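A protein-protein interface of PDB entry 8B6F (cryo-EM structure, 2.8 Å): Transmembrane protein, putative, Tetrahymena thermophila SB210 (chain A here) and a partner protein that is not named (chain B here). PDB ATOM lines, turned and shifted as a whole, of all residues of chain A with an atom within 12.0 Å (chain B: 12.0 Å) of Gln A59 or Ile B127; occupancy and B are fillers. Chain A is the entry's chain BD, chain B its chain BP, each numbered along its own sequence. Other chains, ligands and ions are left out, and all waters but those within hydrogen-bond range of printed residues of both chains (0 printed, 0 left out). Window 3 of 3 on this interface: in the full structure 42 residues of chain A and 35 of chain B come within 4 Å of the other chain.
Of the 11 printed residues of chain A, 8 touch a printed residue of chain B. Hydrophobic or aromatic side chains of chain A that line the printed part of chain B: Met A58, Ala A61 and Tyr A62.
Among the printed residues, merely in contact across the chains: Gln A59 with Lys B125 (2.9 Å), Arg A153 with Pro B121 (3.0 Å), Tyr A62 with Pro B124 (3.2 Å), Glu A64 with Gln B119 (3.3 Å), Met A58 with Ala B126 (3.3 Å), Arg A153 with Pro B124 (3.5 Å), Met A58 with Lys B128 (3.5 Å), Pro A63 with Pro B118 (3.6 Å), Gln A59 with Ile B127 (3.6 Å), Tyr A62 with Pro B118 (3.6 Å), Ala A61 with Ala B126 (3.7 Å), Asn A60 with Gln B119 (3.8 Å), Pro A63 with Gln B119 (3.9 Å), Tyr A62 with Gln B119 (3.9 Å), Met A58 with Ile B127 (3.96 Å) and Asn A60 with Lys B125 (3.99 Å).
Of chain B, only Lys B125, Ala B126 and Ile B127 come within 4 Å of Gln A59. Of chain A, only Met A58 (3.96 Å) and Gln A59 (3.6 Å) come within 4 Å of Ile B127. Of chain B, only Pro B124 (3.4 Å) and Ala B126 (3.7 Å) come within 4 Å of Ala A61. Of chain A, only Met A58 (3.3 Å), Gln A59 (2.5 Å) and Ala A61 (3.7 Å) come within 4 Å of Ala B126. Printed residues of chain A within 4 Å of Pro B121: Arg A153 (3.0 Å). Of the printed residues of chain A, Pro B118 touches Tyr A62 (3.6 Å) and Pro A63 (3.6 Å). Val B122 touches none of the printed residues of chain A. Lys A159 touches none of the printed residues of chain B. The nearest residue of chain A that does not touch Ile B127 is Ala A61 (6.8 Å).
The side-chain carboxylate (OE1) of Glu A148 lies within salt-bridge range of the guanidinium group (NH1) of Arg A153 (3.9 Å). The side-chain carboxylate of Asp B117 sits close to the backbone NH of Gln B119, at 3.4 Å.
The guanidinium group (NH2) of Arg A153 sits at hydrogen-bond distance from the backbone carbonyl oxygen (O) of Ala B123, at 3.2 Å. The backbone NH (N) of Ala A61 lies within hydrogen-bond range of the backbone carbonyl oxygen (O) of Pro B124 (3.4 Å). N of Lys B125 sits close to NH2 of Arg A153, 3.2 Å away. The backbone NH of Ala B126 is in hydrogen-bond range of the backbone carbonyl oxygen of Gln A59, 2.5 Å away. The side-chain sulfur (SD) of Met A58 sits close to the backbone carbonyl oxygen (O) of Lys B125 (3.6 Å).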
ATOM      1  N   MET A  58     -13.679 -32.109 -25.647  1.00  0.00           N
ATOM      2  CA  MET A  58     -13.683 -30.926 -24.742  1.00  0.00           C
ATOM      3  C   MET A  58     -12.403 -30.116 -24.907  1.00  0.00           C
ATOM      4  O   MET A  58     -11.316 -30.677 -25.031  1.00  0.00           O
ATOM      5  CB  MET A  58     -13.838 -31.367 -23.285  1.00  0.00           C
ATOM      6  CG  MET A  58     -15.233 -31.859 -22.924  1.00  0.00           C
ATOM      7  SD  MET A  58     -16.483 -30.564 -23.024  1.00  0.00           S
ATOM      8  CE  MET A  58     -17.868 -31.362 -22.219  1.00  0.00           C
ATOM      9  N   GLN A  59     -12.540 -28.792 -24.905  1.00  0.00           N
ATOM     10  CA  GLN A  59     -11.398 -27.900 -25.026  1.00  0.00           C
ATOM     11  C   GLN A  59     -11.694 -26.619 -24.264  1.00  0.00           C
ATOM     12  O   GLN A  59     -12.853 -26.271 -24.028  1.00  0.00           O
ATOM     13  CB  GLN A  59     -11.076 -27.591 -26.493  1.00  0.00           C
ATOM     14  CG  GLN A  59     -12.225 -26.950 -27.257  1.00  0.00           C
ATOM     15  CD  GLN A  59     -11.866 -26.655 -28.697  1.00  0.00           C
ATOM     16  OE1 GLN A  59     -10.739 -26.892 -29.127  1.00  0.00           O
ATOM     17  NE2 GLN A  59     -12.826 -26.135 -29.451  1.00  0.00           N
ATOM     18  N   ASN A  60     -10.630 -25.915 -23.884  1.00  0.00           N
ATOM     19  CA  ASN A  60     -10.790 -24.686 -23.118  1.00  0.00           C
ATOM     20  C   ASN A  60     -11.619 -23.672 -23.895  1.00  0.00           C
ATOM     21  O   ASN A  60     -11.388 -23.441 -25.085  1.00  0.00           O
ATOM     22  CB  ASN A  60      -9.421 -24.098 -22.776  1.00  0.00           C
ATOM     23  CG  ASN A  60      -8.663 -24.939 -21.771  1.00  0.00           C
ATOM     24  OD1 ASN A  60      -9.260 -25.597 -20.920  1.00  0.00           O
ATOM     25  ND2 ASN A  60      -7.338 -24.921 -21.863  1.00  0.00           N
ATOM     26  N   ALA A  61     -12.588 -23.065 -23.212  1.00  0.00           N
ATOM     27  CA  ALA A  61     -13.483 -22.087 -23.817  1.00  0.00           C
ATOM     28  C   ALA A  61     -13.059 -20.648 -23.558  1.00  0.00           C
ATOM     29  O   ALA A  61     -13.135 -19.813 -24.463  1.00  0.00           O
ATOM     30  CB  ALA A  61     -14.908 -22.294 -23.300  1.00  0.00           C
ATOM     31  N   TYR A  62     -12.617 -20.335 -22.344  1.00  0.00           N
ATOM     32  CA  TYR A  62     -12.209 -18.978 -22.033  1.00  0.00           C
ATOM     33  C   TYR A  62     -10.877 -18.652 -22.706  1.00  0.00           C
ATOM     34  O   TYR A  62     -10.084 -19.549 -23.002  1.00  0.00           O
ATOM     35  CB  TYR A  62     -12.071 -18.791 -20.524  1.00  0.00           C
ATOM     36  CG  TYR A  62     -13.372 -18.835 -19.753  1.00  0.00           C
ATOM     37  CD1 TYR A  62     -14.598 -18.883 -20.408  1.00  0.00           C
ATOM     38  CD2 TYR A  62     -13.372 -18.819 -18.366  1.00  0.00           C
ATOM     39  CE1 TYR A  62     -15.782 -18.917 -19.701  1.00  0.00           C
ATOM     40  CE2 TYR A  62     -14.551 -18.854 -17.651  1.00  0.00           C
ATOM     41  CZ  TYR A  62     -15.752 -18.906 -18.325  1.00  0.00           C
ATOM     42  OH  TYR A  62     -16.930 -18.942 -17.619  1.00  0.00           O
ATOM     43  N   PRO A  63     -10.608 -17.372 -22.965  1.00  0.00           N
ATOM     44  CA  PRO A  63      -9.296 -16.998 -23.499  1.00  0.00           C
ATOM     45  C   PRO A  63      -8.193 -17.290 -22.493  1.00  0.00           C
ATOM     46  O   PRO A  63      -8.394 -17.224 -21.279  1.00  0.00           O
ATOM     47  CB  PRO A  63      -9.434 -15.495 -23.770  1.00  0.00           C
ATOM     48  CG  PRO A  63     -10.537 -15.046 -22.883  1.00  0.00           C
ATOM     49  CD  PRO A  63     -11.485 -16.201 -22.784  1.00  0.00           C
ATOM     50  N   GLU A  64      -7.015 -17.612 -23.015  1.00  0.00           N
ATOM     51  CA  GLU A  64      -5.904 -18.025 -22.175  1.00  0.00           C
ATOM     52  C   GLU A  64      -5.267 -16.827 -21.475  1.00  0.00           C
ATOM     53  O   GLU A  64      -5.398 -15.677 -21.902  1.00  0.00           O
ATOM     54  CB  GLU A  64      -4.851 -18.762 -23.004  1.00  0.00           C
ATOM     55  CG  GLU A  64      -5.383 -20.004 -23.700  1.00  0.00           C
ATOM     56  CD  GLU A  64      -4.306 -20.754 -24.459  1.00  0.00           C
ATOM     57  OE1 GLU A  64      -3.126 -20.354 -24.374  1.00  0.00           O
ATOM     58  OE2 GLU A  64      -4.640 -21.746 -25.141  1.00  0.00           O
ATOM     59  N   GLU A 148     -21.029 -34.602 -15.261  1.00  0.00           N
ATOM     60  CA  GLU A 148     -20.224 -33.469 -14.814  1.00  0.00           C
ATOM     61  C   GLU A 148     -21.143 -32.274 -14.583  1.00  0.00           C
ATOM     62  O   GLU A 148     -21.367 -31.454 -15.475  1.00  0.00           O
ATOM     63  CB  GLU A 148     -19.135 -33.148 -15.831  1.00  0.00           C
ATOM     64  CG  GLU A 148     -18.054 -34.211 -15.921  1.00  0.00           C
ATOM     65  CD  GLU A 148     -17.005 -33.891 -16.966  1.00  0.00           C
ATOM     66  OE1 GLU A 148     -17.128 -32.840 -17.628  1.00  0.00           O
ATOM     67  OE2 GLU A 148     -16.060 -34.690 -17.127  1.00  0.00           O
ATOM     68  N   ARG A 153     -14.077 -31.794 -12.667  1.00  0.00           N
ATOM     69  CA  ARG A 153     -14.214 -32.574 -13.886  1.00  0.00           C
ATOM     70  C   ARG A 153     -13.739 -34.003 -13.661  1.00  0.00           C
ATOM     71  O   ARG A 153     -12.793 -34.256 -12.912  1.00  0.00           O
ATOM     72  CB  ARG A 153     -13.409 -31.947 -15.027  1.00  0.00           C
ATOM     73  CG  ARG A 153     -13.899 -30.583 -15.476  1.00  0.00           C
ATOM     74  CD  ARG A 153     -15.319 -30.648 -16.006  1.00  0.00           C
ATOM     75  NE  ARG A 153     -15.755 -29.368 -16.553  1.00  0.00           N
ATOM     76  CZ  ARG A 153     -15.608 -28.996 -17.817  1.00  0.00           C
ATOM     77  NH1 ARG A 153     -15.027 -29.782 -18.708  1.00  0.00           N
ATOM     78  NH2 ARG A 153     -16.055 -27.804 -18.197  1.00  0.00           N
ATOM     79  N   LYS A 154     -14.407 -34.940 -14.326  1.00  0.00           N
ATOM     80  CA  LYS A 154     -13.992 -36.333 -14.262  1.00  0.00           C
ATOM     81  C   LYS A 154     -12.634 -36.492 -14.932  1.00  0.00           C
ATOM     82  O   LYS A 154     -12.423 -36.022 -16.053  1.00  0.00           O
ATOM     83  CB  LYS A 154     -15.030 -37.226 -14.939  1.00  0.00           C
ATOM     84  CG  LYS A 154     -16.426 -37.120 -14.342  1.00  0.00           C
ATOM     85  CD  LYS A 154     -16.466 -37.616 -12.905  1.00  0.00           C
ATOM     86  CE  LYS A 154     -17.871 -37.536 -12.331  1.00  0.00           C
ATOM     87  NZ  LYS A 154     -17.935 -38.081 -10.947  1.00  0.00           N
ATOM     88  N   LYS A 159     -12.701 -41.841 -15.839  1.00  0.00           N
ATOM     89  CA  LYS A 159     -13.348 -42.268 -17.074  1.00  0.00           C
ATOM     90  C   LYS A 159     -12.913 -43.675 -17.465  1.00  0.00           C
ATOM     91  O   LYS A 159     -13.719 -44.460 -17.977  1.00  0.00           O
ATOM     92  CB  LYS A 159     -13.056 -41.274 -18.196  1.00  0.00           C
ATOM     93  CG  LYS A 159     -13.991 -40.072 -18.189  1.00  0.00           C
ATOM     94  CD  LYS A 159     -13.586 -39.020 -19.207  1.00  0.00           C
ATOM     95  CE  LYS A 159     -12.376 -38.234 -18.738  1.00  0.00           C
ATOM     96  NZ  LYS A 159     -12.064 -37.097 -19.648  1.00  0.00           N
ATOM     97  N   ASP B 117      -9.282 -19.961 -12.641  1.00  0.00           N
ATOM     98  CA  ASP B 117      -8.257 -19.993 -13.674  1.00  0.00           C
ATOM     99  C   ASP B 117      -8.869 -20.498 -14.975  1.00  0.00           C
ATOM    100  O   ASP B 117      -9.423 -21.604 -14.996  1.00  0.00           O
ATOM    101  CB  ASP B 117      -7.105 -20.889 -13.237  1.00  0.00           C
ATOM    102  CG  ASP B 117      -6.003 -20.966 -14.268  1.00  0.00           C
ATOM    103  OD1 ASP B 117      -5.335 -19.939 -14.505  1.00  0.00           O
ATOM    104  OD2 ASP B 117      -5.799 -22.054 -14.839  1.00  0.00           O
ATOM    105  N   PRO B 118      -8.799 -19.742 -16.074  1.00  0.00           N
ATOM    106  CA  PRO B 118      -9.484 -20.186 -17.299  1.00  0.00           C
ATOM    107  C   PRO B 118      -8.985 -21.517 -17.834  1.00  0.00           C
ATOM    108  O   PRO B 118      -9.751 -22.229 -18.495  1.00  0.00           O
ATOM    109  CB  PRO B 118      -9.215 -19.039 -18.285  1.00  0.00           C
ATOM    110  CG  PRO B 118      -8.007 -18.357 -17.764  1.00  0.00           C
ATOM    111  CD  PRO B 118      -8.077 -18.474 -16.277  1.00  0.00           C
ATOM    112  N   GLN B 119      -7.729 -21.875 -17.580  1.00  0.00           N
ATOM    113  CA  GLN B 119      -7.162 -23.120 -18.083  1.00  0.00           C
ATOM    114  C   GLN B 119      -7.296 -24.281 -17.107  1.00  0.00           C
ATOM    115  O   GLN B 119      -6.900 -25.401 -17.444  1.00  0.00           O
ATOM    116  CB  GLN B 119      -5.685 -22.922 -18.439  1.00  0.00           C
ATOM    117  CG  GLN B 119      -5.460 -22.299 -19.810  1.00  0.00           C
ATOM    118  CD  GLN B 119      -6.113 -20.941 -19.953  1.00  0.00           C
ATOM    119  OE1 GLN B 119      -5.573 -19.930 -19.508  1.00  0.00           O
ATOM    120  NE2 GLN B 119      -7.284 -20.911 -20.578  1.00  0.00           N
ATOM    121  N   SER B 120      -7.834 -24.052 -15.913  1.00  0.00           N
ATOM    122  CA  SER B 120      -8.027 -25.143 -14.976  1.00  0.00           C
ATOM    123  C   SER B 120      -9.143 -26.058 -15.478  1.00  0.00           C
ATOM    124  O   SER B 120     -10.038 -25.616 -16.201  1.00  0.00           O
ATOM    125  CB  SER B 120      -8.369 -24.611 -13.588  1.00  0.00           C
ATOM    126  OG  SER B 120      -9.538 -23.813 -13.619  1.00  0.00           O
ATOM    127  N   PRO B 121      -9.115 -27.342 -15.109  1.00  0.00           N
ATOM    128  CA  PRO B 121     -10.177 -28.246 -15.577  1.00  0.00           C
ATOM    129  C   PRO B 121     -11.572 -27.793 -15.188  1.00  0.00           C
ATOM    130  O   PRO B 121     -12.517 -27.993 -15.960  1.00  0.00           O
ATOM    131  CB  PRO B 121      -9.813 -29.582 -14.915  1.00  0.00           C
ATOM    132  CG  PRO B 121      -8.354 -29.491 -14.650  1.00  0.00           C
ATOM    133  CD  PRO B 121      -8.087 -28.054 -14.331  1.00  0.00           C
ATOM    134  N   VAL B 122     -11.731 -27.184 -14.012  1.00  0.00           N
ATOM    135  CA  VAL B 122     -13.052 -26.763 -13.556  1.00  0.00           C
ATOM    136  C   VAL B 122     -13.631 -25.690 -14.462  1.00  0.00           C
ATOM    137  O   VAL B 122     -14.855 -25.549 -14.566  1.00  0.00           O
ATOM    138  CB  VAL B 122     -12.973 -26.288 -12.096  1.00  0.00           C
ATOM    139  CG1 VAL B 122     -14.324 -25.776 -11.611  1.00  0.00           C
ATOM    140  CG2 VAL B 122     -12.498 -27.417 -11.232  1.00  0.00           C
ATOM    141  N   ALA B 123     -12.778 -24.915 -15.122  1.00  0.00           N
ATOM    142  CA  ALA B 123     -13.272 -23.869 -15.996  1.00  0.00           C
ATOM    143  C   ALA B 123     -14.069 -24.487 -17.143  1.00  0.00           C
ATOM    144  O   ALA B 123     -13.757 -25.589 -17.603  1.00  0.00           O
ATOM    145  CB  ALA B 123     -12.113 -23.042 -16.548  1.00  0.00           C
ATOM    146  N   PRO B 124     -15.102 -23.801 -17.625  1.00  0.00           N
ATOM    147  CA  PRO B 124     -15.928 -24.377 -18.693  1.00  0.00           C
ATOM    148  C   PRO B 124     -15.109 -24.660 -19.942  1.00  0.00           C
ATOM    149  O   PRO B 124     -14.185 -23.922 -20.286  1.00  0.00           O
ATOM    150  CB  PRO B 124     -16.991 -23.299 -18.942  1.00  0.00           C
ATOM    151  CG  PRO B 124     -16.397 -22.048 -18.422  1.00  0.00           C
ATOM    152  CD  PRO B 124     -15.542 -22.444 -17.263  1.00  0.00           C
ATOM    153  N   LYS B 125     -15.460 -25.751 -20.619  1.00  0.00           N
ATOM    154  CA  LYS B 125     -14.749 -26.213 -21.801  1.00  0.00           C
ATOM    155  C   LYS B 125     -15.729 -26.365 -22.953  1.00  0.00           C
ATOM    156  O   LYS B 125     -16.809 -26.939 -22.781  1.00  0.00           O
ATOM    157  CB  LYS B 125     -14.040 -27.546 -21.533  1.00  0.00           C
ATOM    158  CG  LYS B 125     -12.972 -27.470 -20.455  1.00  0.00           C
ATOM    159  CD  LYS B 125     -12.218 -28.784 -20.326  1.00  0.00           C
ATOM    160  CE  LYS B 125     -11.142 -28.695 -19.257  1.00  0.00           C
ATOM    161  NZ  LYS B 125     -10.373 -29.965 -19.128  1.00  0.00           N
ATOM    162  N   ALA B 126     -15.354 -25.849 -24.118  1.00  0.00           N
ATOM    163  CA  ALA B 126     -16.193 -25.954 -25.298  1.00  0.00           C
ATOM    164  C   ALA B 126     -16.075 -27.345 -25.917  1.00  0.00           C
ATOM    165  O   ALA B 126     -15.105 -28.073 -25.696  1.00  0.00           O
ATOM    166  CB  ALA B 126     -15.809 -24.889 -26.324  1.00  0.00           C
ATOM    167  N   ILE B 127     -17.087 -27.708 -26.706  1.00  0.00           N
ATOM    168  CA  ILE B 127     -17.097 -29.008 -27.364  1.00  0.00           C
ATOM    169  C   ILE B 127     -16.037 -29.032 -28.457  1.00  0.00           C
ATOM    170  O   ILE B 127     -15.882 -28.072 -29.222  1.00  0.00           O
ATOM    171  CB  ILE B 127     -18.492 -29.311 -27.937  1.00  0.00           C
ATOM    172  CG1 ILE B 127     -19.552 -29.296 -26.832  1.00  0.00           C
ATOM    173  CG2 ILE B 127     -18.496 -30.652 -28.661  1.00  0.00           C
ATOM    174  CD1 ILE B 127     -19.345 -30.332 -25.745  1.00  0.00           C
ATOM    175  N   LYS B 128     -15.299 -30.137 -28.532  1.00  0.00           N
ATOM    176  CA  LYS B 128     -14.257 -30.328 -29.535  1.00  0.00           C
ATOM    177  C   LYS B 128     -14.784 -31.289 -30.594  1.00  0.00           C
ATOM    178  O   LYS B 128     -14.982 -32.477 -30.321  1.00  0.00           O
ATOM    179  CB  LYS B 128     -12.979 -30.861 -28.894  1.00  0.00           C
ATOM    180  CG  LYS B 128     -11.831 -31.057 -29.868  1.00  0.00           C
ATOM    181  CD  LYS B 128     -10.600 -31.586 -29.153  1.00  0.00           C
ATOM    182  CE  LYS B 128      -9.434 -31.756 -30.110  1.00  0.00           C
ATOM    183  NZ  LYS B 128      -8.220 -32.266 -29.413  1.00  0.00           N
ATOM    184  N   TYR B 129     -15.009 -30.776 -31.799  1.00  0.00           N
ATOM    185  CA  TYR B 129     -15.541 -31.584 -32.888  1.00  0.00           C
ATOM    186  C   TYR B 129     -14.507 -32.595 -33.369  1.00  0.00           C
ATOM    187  O   TYR B 129     -14.822 -33.511 -34.127  1.00  0.00           O
ATOM    188  CB  TYR B 129     -15.979 -30.694 -34.054  1.00  0.00           C
ATOM    189  CG  TYR B 129     -16.988 -29.632 -33.679  1.00  0.00           C
ATOM    190  CD1 TYR B 129     -17.889 -29.832 -32.641  1.00  0.00           C
ATOM    191  CD2 TYR B 129     -17.036 -28.426 -34.365  1.00  0.00           C
ATOM    192  CE1 TYR B 129     -18.810 -28.860 -32.299  1.00  0.00           C
ATOM    193  CE2 TYR B 129     -17.952 -27.450 -34.030  1.00  0.00           C
ATOM    194  CZ  TYR B 129     -18.836 -27.672 -32.998  1.00  0.00           C
ATOM    195  OH  TYR B 129     -19.748 -26.700 -32.665  1.00  0.00           O
ATOM    196  OXT TYR B 129     -13.331 -32.515 -33.013  1.00  0.00           O
